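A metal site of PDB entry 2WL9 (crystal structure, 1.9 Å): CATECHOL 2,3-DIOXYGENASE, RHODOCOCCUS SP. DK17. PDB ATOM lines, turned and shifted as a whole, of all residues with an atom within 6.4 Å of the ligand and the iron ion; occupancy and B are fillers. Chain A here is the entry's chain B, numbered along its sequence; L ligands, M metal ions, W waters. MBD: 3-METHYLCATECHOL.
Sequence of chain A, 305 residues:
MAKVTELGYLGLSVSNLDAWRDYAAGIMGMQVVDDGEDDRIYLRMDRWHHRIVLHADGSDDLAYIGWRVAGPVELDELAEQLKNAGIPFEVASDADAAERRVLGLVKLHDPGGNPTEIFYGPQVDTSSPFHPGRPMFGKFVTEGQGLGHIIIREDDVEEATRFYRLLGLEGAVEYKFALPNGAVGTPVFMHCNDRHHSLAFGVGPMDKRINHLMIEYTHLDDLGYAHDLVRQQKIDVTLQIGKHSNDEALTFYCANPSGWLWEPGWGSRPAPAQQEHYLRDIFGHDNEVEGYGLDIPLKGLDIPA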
ATOM      1  N   HIS A 149     -32.950  -8.946  25.860  1.00  0.00           N
ATOM      2  CA  HIS A 149     -32.154  -9.026  24.634  1.00  0.00           C
ATOM      3  C   HIS A 149     -32.822  -9.841  23.539  1.00  0.00           C
ATOM      4  O   HIS A 149     -33.687 -10.676  23.806  1.00  0.00           O
ATOM      5  CB  HIS A 149     -30.726  -9.539  24.886  1.00  0.00           C
ATOM      6  CG  HIS A 149     -30.634 -10.999  25.208  1.00  0.00           C
ATOM      7  ND1 HIS A 149     -30.238 -11.449  26.448  1.00  0.00           N
ATOM      8  CD2 HIS A 149     -30.833 -12.097  24.440  1.00  0.00           C
ATOM      9  CE1 HIS A 149     -30.216 -12.775  26.442  1.00  0.00           C
ATOM     10  NE2 HIS A 149     -30.556 -13.194  25.239  1.00  0.00           N
ATOM     11  N   ILE A 151     -32.237 -11.833  19.506  1.00  0.00           N
ATOM     12  CA  ILE A 151     -31.414 -12.297  18.414  1.00  0.00           C
ATOM     13  C   ILE A 151     -32.224 -12.060  17.164  1.00  0.00           C
ATOM     14  O   ILE A 151     -33.367 -12.491  17.076  1.00  0.00           O
ATOM     15  CB  ILE A 151     -31.028 -13.783  18.545  1.00  0.00           C
ATOM     16  CG1 ILE A 151     -29.924 -13.946  19.598  1.00  0.00           C
ATOM     17  CG2 ILE A 151     -30.584 -14.352  17.181  1.00  0.00           C
ATOM     18  CD1 ILE A 151     -29.167 -15.282  19.527  1.00  0.00           C
ATOM     19  N   GLU A 174     -18.627 -14.239  20.417  1.00  0.00           N
ATOM     20  CA  GLU A 174     -18.449 -14.821  21.753  1.00  0.00           C
ATOM     21  C   GLU A 174     -18.532 -16.340  21.776  1.00  0.00           C
ATOM     22  O   GLU A 174     -18.180 -16.974  22.774  1.00  0.00           O
ATOM     23  CB  GLU A 174     -19.445 -14.222  22.756  1.00  0.00           C
ATOM     24  CG  GLU A 174     -19.000 -12.880  23.308  1.00  0.00           C
ATOM     25  CD  GLU A 174     -19.969 -12.285  24.318  1.00  0.00           C
ATOM     26  OE1 GLU A 174     -19.686 -11.182  24.808  1.00  0.00           O
ATOM     27  OE2 GLU A 174     -21.017 -12.907  24.605  1.00  0.00           O
ATOM     28  N   TYR A 175     -18.968 -16.927  20.664  1.00  0.00           N
ATOM     29  CA  TYR A 175     -19.081 -18.374  20.551  1.00  0.00           C
ATOM     30  C   TYR A 175     -18.482 -18.879  19.247  1.00  0.00           C
ATOM     31  O   TYR A 175     -18.639 -18.257  18.198  1.00  0.00           O
ATOM     32  CB  TYR A 175     -20.548 -18.806  20.641  1.00  0.00           C
ATOM     33  CG  TYR A 175     -20.996 -19.268  22.018  1.00  0.00           C
ATOM     34  CD1 TYR A 175     -21.153 -20.623  22.305  1.00  0.00           C
ATOM     35  CD2 TYR A 175     -21.255 -18.342  23.030  1.00  0.00           C
ATOM     36  CE1 TYR A 175     -21.555 -21.057  23.569  1.00  0.00           C
ATOM     37  CE2 TYR A 175     -21.666 -18.762  24.312  1.00  0.00           C
ATOM     38  CZ  TYR A 175     -21.809 -20.110  24.571  1.00  0.00           C
ATOM     39  OH  TYR A 175     -22.212 -20.541  25.814  1.00  0.00           O
ATOM     40  N   PRO A 187     -21.655 -16.386  16.446  1.00  0.00           N
ATOM     41  CA  PRO A 187     -22.625 -15.353  16.770  1.00  0.00           C
ATOM     42  C   PRO A 187     -21.940 -14.184  17.483  1.00  0.00           C
ATOM     43  O   PRO A 187     -21.020 -14.393  18.277  1.00  0.00           O
ATOM     44  CB  PRO A 187     -23.617 -16.055  17.704  1.00  0.00           C
ATOM     45  CG  PRO A 187     -23.298 -17.501  17.623  1.00  0.00           C
ATOM     46  CD  PRO A 187     -21.861 -17.599  17.264  1.00  0.00           C
ATOM     47  N   PHE A 189     -22.303 -10.822  19.892  1.00  0.00           N
ATOM     48  CA  PHE A 189     -23.130 -10.383  21.017  1.00  0.00           C
ATOM     49  C   PHE A 189     -22.746  -8.954  21.360  1.00  0.00           C
ATOM     50  O   PHE A 189     -21.558  -8.627  21.419  1.00  0.00           O
ATOM     51  CB  PHE A 189     -22.914 -11.316  22.201  1.00  0.00           C
ATOM     52  CG  PHE A 189     -23.406 -12.721  21.977  1.00  0.00           C
ATOM     53  CD1 PHE A 189     -24.621 -13.138  22.509  1.00  0.00           C
ATOM     54  CD2 PHE A 189     -22.659 -13.630  21.224  1.00  0.00           C
ATOM     55  CE1 PHE A 189     -25.093 -14.428  22.294  1.00  0.00           C
ATOM     56  CE2 PHE A 189     -23.124 -14.927  21.007  1.00  0.00           C
ATOM     57  CZ  PHE A 189     -24.332 -15.327  21.551  1.00  0.00           C
ATOM     58  N   HIS A 196     -25.654  -8.071  30.030  1.00  0.00           N
ATOM     59  CA  HIS A 196     -24.549  -8.755  29.370  1.00  0.00           C
ATOM     60  C   HIS A 196     -24.556  -8.476  27.868  1.00  0.00           C
ATOM     61  O   HIS A 196     -23.535  -8.122  27.287  1.00  0.00           O
ATOM     62  CB  HIS A 196     -24.598 -10.258  29.588  1.00  0.00           C
ATOM     63  CG  HIS A 196     -23.515 -10.976  28.855  1.00  0.00           C
ATOM     64  ND1 HIS A 196     -23.603 -11.290  27.518  1.00  0.00           N
ATOM     65  CD2 HIS A 196     -22.286 -11.376  29.257  1.00  0.00           C
ATOM     66  CE1 HIS A 196     -22.481 -11.882  27.135  1.00  0.00           C
ATOM     67  NE2 HIS A 196     -21.679 -11.952  28.178  1.00  0.00           N
ATOM     68  N   HIS A 197     -25.712  -8.687  27.245  1.00  0.00           N
ATOM     69  CA  HIS A 197     -25.938  -8.230  25.887  1.00  0.00           C
ATOM     70  C   HIS A 197     -27.397  -7.814  25.679  1.00  0.00           C
ATOM     71  O   HIS A 197     -28.292  -8.265  26.413  1.00  0.00           O
ATOM     72  CB  HIS A 197     -25.454  -9.254  24.835  1.00  0.00           C
ATOM     73  CG  HIS A 197     -26.117 -10.599  24.918  1.00  0.00           C
ATOM     74  ND1 HIS A 197     -27.033 -11.028  23.985  1.00  0.00           N
ATOM     75  CD2 HIS A 197     -25.976 -11.606  25.803  1.00  0.00           C
ATOM     76  CE1 HIS A 197     -27.438 -12.247  24.300  1.00  0.00           C
ATOM     77  NE2 HIS A 197     -26.815 -12.617  25.408  1.00  0.00           N
ATOM     78  N   ALA A 200     -27.882  -9.869  19.694  1.00  0.00           N
ATOM     79  CA  ALA A 200     -26.998 -10.845  19.066  1.00  0.00           C
ATOM     80  C   ALA A 200     -27.479 -11.211  17.658  1.00  0.00           C
ATOM     81  O   ALA A 200     -28.638 -11.009  17.313  1.00  0.00           O
ATOM     82  CB  ALA A 200     -26.876 -12.079  19.942  1.00  0.00           C
ATOM     83  N   VAL A 203     -26.629 -16.298  13.588  1.00  0.00           N
ATOM     84  CA  VAL A 203     -26.997 -17.642  14.049  1.00  0.00           C
ATOM     85  C   VAL A 203     -27.344 -18.596  12.888  1.00  0.00           C
ATOM     86  O   VAL A 203     -27.661 -19.768  13.115  1.00  0.00           O
ATOM     87  CB  VAL A 203     -28.124 -17.621  15.126  1.00  0.00           C
ATOM     88  CG1 VAL A 203     -27.745 -16.723  16.303  1.00  0.00           C
ATOM     89  CG2 VAL A 203     -29.464 -17.188  14.541  1.00  0.00           C
ATOM     90  N   ASN A 211     -35.266 -14.379  16.240  1.00  0.00           N
ATOM     91  CA  ASN A 211     -35.192 -15.724  16.782  1.00  0.00           C
ATOM     92  C   ASN A 211     -35.788 -15.814  18.180  1.00  0.00           C
ATOM     93  O   ASN A 211     -36.668 -16.644  18.422  1.00  0.00           O
ATOM     94  CB  ASN A 211     -33.753 -16.245  16.810  1.00  0.00           C
ATOM     95  CG  ASN A 211     -33.649 -17.651  17.376  1.00  0.00           C
ATOM     96  OD1 ASN A 211     -34.071 -18.629  16.742  1.00  0.00           O
ATOM     97  ND2 ASN A 211     -33.090 -17.766  18.576  1.00  0.00           N
ATOM     98  N   HIS A 212     -35.292 -14.982  19.089  1.00  0.00           N
ATOM     99  CA  HIS A 212     -35.835 -14.968  20.442  1.00  0.00           C
ATOM    100  C   HIS A 212     -35.671 -13.636  21.147  1.00  0.00           C
ATOM    101  O   HIS A 212     -34.882 -12.794  20.717  1.00  0.00           O
ATOM    102  CB  HIS A 212     -35.249 -16.118  21.299  1.00  0.00           C
ATOM    103  CG  HIS A 212     -33.862 -15.872  21.813  1.00  0.00           C
ATOM    104  ND1 HIS A 212     -32.731 -16.151  21.083  1.00  0.00           N
ATOM    105  CD2 HIS A 212     -33.431 -15.392  23.007  1.00  0.00           C
ATOM    106  CE1 HIS A 212     -31.662 -15.851  21.808  1.00  0.00           C
ATOM    107  NE2 HIS A 212     -32.064 -15.391  22.973  1.00  0.00           N
ATOM    108  N   MET A 214     -35.135 -12.596  25.263  1.00  0.00           N
ATOM    109  CA  MET A 214     -34.863 -13.037  26.622  1.00  0.00           C
ATOM    110  C   MET A 214     -35.446 -12.031  27.586  1.00  0.00           C
ATOM    111  O   MET A 214     -35.234 -10.827  27.448  1.00  0.00           O
ATOM    112  CB  MET A 214     -33.355 -13.151  26.818  1.00  0.00           C
ATOM    113  CG  MET A 214     -32.909 -13.719  28.176  1.00  0.00           C
ATOM    114  SD  MET A 214     -32.767 -12.456  29.461  1.00  0.00           S
ATOM    115  CE  MET A 214     -32.139 -13.453  30.813  1.00  0.00           C
ATOM    116  N   LEU A 239     -34.908 -25.660  24.286  1.00  0.00           N
ATOM    117  CA  LEU A 239     -33.681 -25.808  25.057  1.00  0.00           C
ATOM    118  C   LEU A 239     -34.049 -25.796  26.536  1.00  0.00           C
ATOM    119  O   LEU A 239     -34.544 -24.796  27.030  1.00  0.00           O
ATOM    120  CB  LEU A 239     -32.711 -24.657  24.768  1.00  0.00           C
ATOM    121  CG  LEU A 239     -32.015 -24.578  23.407  1.00  0.00           C
ATOM    122  CD1 LEU A 239     -30.978 -23.469  23.470  1.00  0.00           C
ATOM    123  CD2 LEU A 239     -31.346 -25.887  23.028  1.00  0.00           C
ATOM    124  N   HIS A 244     -25.687 -20.444  29.680  1.00  0.00           N
ATOM    125  CA  HIS A 244     -24.686 -20.098  28.677  1.00  0.00           C
ATOM    126  C   HIS A 244     -23.413 -19.626  29.381  1.00  0.00           C
ATOM    127  O   HIS A 244     -23.471 -19.074  30.482  1.00  0.00           O
ATOM    128  CB  HIS A 244     -25.198 -19.011  27.728  1.00  0.00           C
ATOM    129  CG  HIS A 244     -26.356 -19.439  26.882  1.00  0.00           C
ATOM    130  ND1 HIS A 244     -26.264 -20.407  25.901  1.00  0.00           N
ATOM    131  CD2 HIS A 244     -27.640 -18.991  26.842  1.00  0.00           C
ATOM    132  CE1 HIS A 244     -27.437 -20.558  25.317  1.00  0.00           C
ATOM    133  NE2 HIS A 244     -28.288 -19.714  25.861  1.00  0.00           N
ATOM    134  N   SER A 245     -22.271 -19.860  28.749  1.00  0.00           N
ATOM    135  CA  SER A 245     -21.003 -19.452  29.348  1.00  0.00           C
ATOM    136  C   SER A 245     -20.815 -17.936  29.345  1.00  0.00           C
ATOM    137  O   SER A 245     -20.124 -17.410  30.200  1.00  0.00           O
ATOM    138  CB  SER A 245     -19.827 -20.150  28.667  1.00  0.00           C
ATOM    139  OG  SER A 245     -19.784 -21.510  29.026  1.00  0.00           O
ATOM    140  N   ASN A 246     -21.434 -17.232  28.393  1.00  0.00           N
ATOM    141  CA  ASN A 246     -21.240 -15.782  28.334  1.00  0.00           C
ATOM    142  C   ASN A 246     -22.005 -15.005  29.412  1.00  0.00           C
ATOM    143  O   ASN A 246     -21.385 -14.363  30.258  1.00  0.00           O
ATOM    144  CB  ASN A 246     -21.476 -15.211  26.927  1.00  0.00           C
ATOM    145  CG  ASN A 246     -22.859 -15.489  26.385  1.00  0.00           C
ATOM    146  OD1 ASN A 246     -23.606 -16.276  26.939  1.00  0.00           O
ATOM    147  ND2 ASN A 246     -23.202 -14.821  25.278  1.00  0.00           N
ATOM    148  N   ASP A 247     -23.339 -15.076  29.396  1.00  0.00           N
ATOM    149  CA  ASP A 247     -24.137 -14.318  30.359  1.00  0.00           C
ATOM    150  C   ASP A 247     -24.200 -14.987  31.736  1.00  0.00           C
ATOM    151  O   ASP A 247     -24.481 -14.318  32.733  1.00  0.00           O
ATOM    152  CB  ASP A 247     -25.548 -13.967  29.837  1.00  0.00           C
ATOM    153  CG  ASP A 247     -26.311 -15.170  29.305  1.00  0.00           C
ATOM    154  OD1 ASP A 247     -25.941 -16.325  29.583  1.00  0.00           O
ATOM    155  OD2 ASP A 247     -27.312 -14.940  28.579  1.00  0.00           O
ATOM    156  N   THR A 251     -31.433 -20.041  32.302  1.00  0.00           N
ATOM    157  CA  THR A 251     -32.556 -19.798  31.368  1.00  0.00           C
ATOM    158  C   THR A 251     -33.078 -21.071  30.686  1.00  0.00           C
ATOM    159  O   THR A 251     -32.402 -22.102  30.657  1.00  0.00           O
ATOM    160  CB  THR A 251     -32.177 -18.794  30.223  1.00  0.00           C
ATOM    161  OG1 THR A 251     -31.535 -19.492  29.148  1.00  0.00           O
ATOM    162  CG2 THR A 251     -31.282 -17.648  30.696  1.00  0.00           C
ATOM    163  N   TYR A 253     -35.577 -21.956  26.862  1.00  0.00           N
ATOM    164  CA  TYR A 253     -36.123 -21.362  25.651  1.00  0.00           C
ATOM    165  C   TYR A 253     -37.420 -22.055  25.256  1.00  0.00           C
ATOM    166  O   TYR A 253     -37.420 -23.271  25.043  1.00  0.00           O
ATOM    167  CB  TYR A 253     -35.133 -21.499  24.504  1.00  0.00           C
ATOM    168  CG  TYR A 253     -33.862 -20.686  24.566  1.00  0.00           C
ATOM    169  CD1 TYR A 253     -33.683 -19.593  23.734  1.00  0.00           C
ATOM    170  CD2 TYR A 253     -32.806 -21.045  25.417  1.00  0.00           C
ATOM    171  CE1 TYR A 253     -32.518 -18.857  23.745  1.00  0.00           C
ATOM    172  CE2 TYR A 253     -31.631 -20.302  25.447  1.00  0.00           C
ATOM    173  CZ  TYR A 253     -31.493 -19.217  24.598  1.00  0.00           C
ATOM    174  OH  TYR A 253     -30.342 -18.466  24.612  1.00  0.00           O
ATOM    175  N   GLU A 263     -37.195 -16.506  25.970  1.00  0.00           N
ATOM    176  CA  GLU A 263     -36.213 -17.123  26.837  1.00  0.00           C
ATOM    177  C   GLU A 263     -36.304 -16.500  28.224  1.00  0.00           C
ATOM    178  O   GLU A 263     -35.624 -15.505  28.512  1.00  0.00           O
ATOM    179  CB  GLU A 263     -34.809 -16.960  26.241  1.00  0.00           C
ATOM    180  CG  GLU A 263     -33.656 -17.547  27.084  1.00  0.00           C
ATOM    181  CD  GLU A 263     -32.293 -17.008  26.700  1.00  0.00           C
ATOM    182  OE1 GLU A 263     -32.218 -16.062  25.886  1.00  0.00           O
ATOM    183  OE2 GLU A 263     -31.270 -17.521  27.223  1.00  0.00           O
ATOM    184  N   ASP A 281     -21.777 -24.222  26.473  1.00  0.00           N
ATOM    185  CA  ASP A 281     -22.534 -23.737  27.632  1.00  0.00           C
ATOM    186  C   ASP A 281     -21.989 -24.364  28.920  1.00  0.00           C
ATOM    187  O   ASP A 281     -21.266 -25.358  28.867  1.00  0.00           O
ATOM    188  CB  ASP A 281     -24.017 -24.112  27.466  1.00  0.00           C
ATOM    189  CG  ASP A 281     -24.726 -23.276  26.414  1.00  0.00           C
ATOM    190  OD1 ASP A 281     -24.148 -22.293  25.898  1.00  0.00           O
ATOM    191  OD2 ASP A 281     -25.897 -23.602  26.114  1.00  0.00           O
ATOM    192  N   LEU A 294     -32.644 -22.931  16.785  1.00  0.00           N
ATOM    193  CA  LEU A 294     -31.569 -23.087  17.751  1.00  0.00           C
ATOM    194  C   LEU A 294     -31.238 -24.561  17.965  1.00  0.00           C
ATOM    195  O   LEU A 294     -31.013 -24.996  19.100  1.00  0.00           O
ATOM    196  CB  LEU A 294     -31.935 -22.421  19.085  1.00  0.00           C
ATOM    197  CG  LEU A 294     -31.989 -20.892  19.177  1.00  0.00           C
ATOM    198  CD1 LEU A 294     -32.582 -20.490  20.522  1.00  0.00           C
ATOM    199  CD2 LEU A 294     -30.615 -20.262  18.998  1.00  0.00           C
ATOM    200  N   LEU A 298     -24.954 -27.591  22.119  1.00  0.00           N
ATOM    201  CA  LEU A 298     -24.312 -26.535  22.911  1.00  0.00           C
ATOM    202  C   LEU A 298     -23.374 -27.050  24.006  1.00  0.00           C
ATOM    203  O   LEU A 298     -22.770 -26.255  24.730  1.00  0.00           O
ATOM    204  CB  LEU A 298     -25.370 -25.607  23.505  1.00  0.00           C
ATOM    205  CG  LEU A 298     -25.983 -24.575  22.553  1.00  0.00           C
ATOM    206  CD1 LEU A 298     -27.367 -24.160  23.040  1.00  0.00           C
ATOM    207  CD2 LEU A 298     -25.081 -23.355  22.420  1.00  0.00           C
HETATM  208  CA1 MBD L   1     -26.101 -16.816  24.890  1.00  0.00           C
HETATM  209  OA1 MBD L   1     -26.179 -15.802  25.783  1.00  0.00           O
HETATM  210  CA2 MBD L   1     -27.192 -17.068  23.925  1.00  0.00           C
HETATM  211  OA2 MBD L   1     -28.288 -16.256  23.939  1.00  0.00           O
HETATM  212  CA3 MBD L   1     -27.065 -18.132  23.021  1.00  0.00           C
HETATM  213  CB3 MBD L   1     -28.147 -18.437  22.019  1.00  0.00           C
HETATM  214  CA4 MBD L   1     -25.931 -18.930  23.039  1.00  0.00           C
HETATM  215  CA5 MBD L   1     -24.900 -18.693  23.942  1.00  0.00           C
HETATM  216  CA6 MBD L   1     -24.988 -17.651  24.858  1.00  0.00           C
HETATM  217 FE    FE M   1     -30.289 -15.672  24.660  1.00  0.00          FE
HETATM  218  O   HOH W   1     -29.018 -15.908  26.800  1.00  0.00           O
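Water W1 lies within hydrogen-bond range of OD2 of Asp 247 (2.6 Å), OE2 of Glu 263 (2.8 Å) and OA1 of the ligand (3.0 Å).
The side-chain carboxylate of Glu 263 sits at hydrogen-bond distance from the side-chain hydroxyl of Tyr 253. The side-chain hydroxyl (OH) of Tyr 175 sits at hydrogen-bond distance from the backbone NH (N) of Ser 245, 3.0 Å away. A ring nitrogen (ND1) of His 212 lies within hydrogen-bond range of the side-chain amide nitrogen of Asn 211, at 3.0 Å. A ring nitrogen (NE2) of His 244 sits at hydrogen-bond distance from the side-chain hydroxyl of Tyr 253. The side-chain hydroxyl (OH) of Tyr 175 sits at hydrogen-bond distance from the side-chain carboxylate (OD1) of Asp 281. O of Asn 246 lies within hydrogen-bond range of NE2 of His 196 (3.2 Å). OE2 of Glu 263 is in hydrogen-bond range of OG1 of Thr 251 (2.8 Å). N of Tyr 253 is in hydrogen-bond range of O of Leu 239, at 3.0 Å.
CE2 of Tyr 175 touches CA5 of the ligand (3.3 Å). Phe 189 touches the ligand. His 244 touches the ligand (ND1 to CA5, 2.9 Å). Hydrophobic or aromatic side chains that line the ligand: Tyr 175, Phe 189 and His 244. The nearest printed residue that does not touch the ligand is His 149 (4.03 Å).
The iron ion is bound by OA2 of the ligand (2.2 Å), OE1 of Glu 263 (2.3 Å), NE2 of His 212 (2.5 Å), water W1 (2.5 Å) and NE2 of His 149 (2.6 Å). Slightly farther from the iron ion lies the side-chain hydroxyl (OH) of Tyr 253 (2.8 Å).
OD2 of Asp 247 is in hydrogen-bond range of OA1 of the ligand (3.1 Å). A ring nitrogen (NE2) of His 197 sits at hydrogen-bond distance from an oxygen (OA1) of the ligand. OH of Tyr 253 lies close to OA2 of the ligand (3.1 Å). The side-chain amide oxygen (OD1) of Asn 246 sits close to an oxygen (OA1) of the ligand, at 2.9 Å.
Of the 24 residues printed, 4 come within 4 Å of the iron ion.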
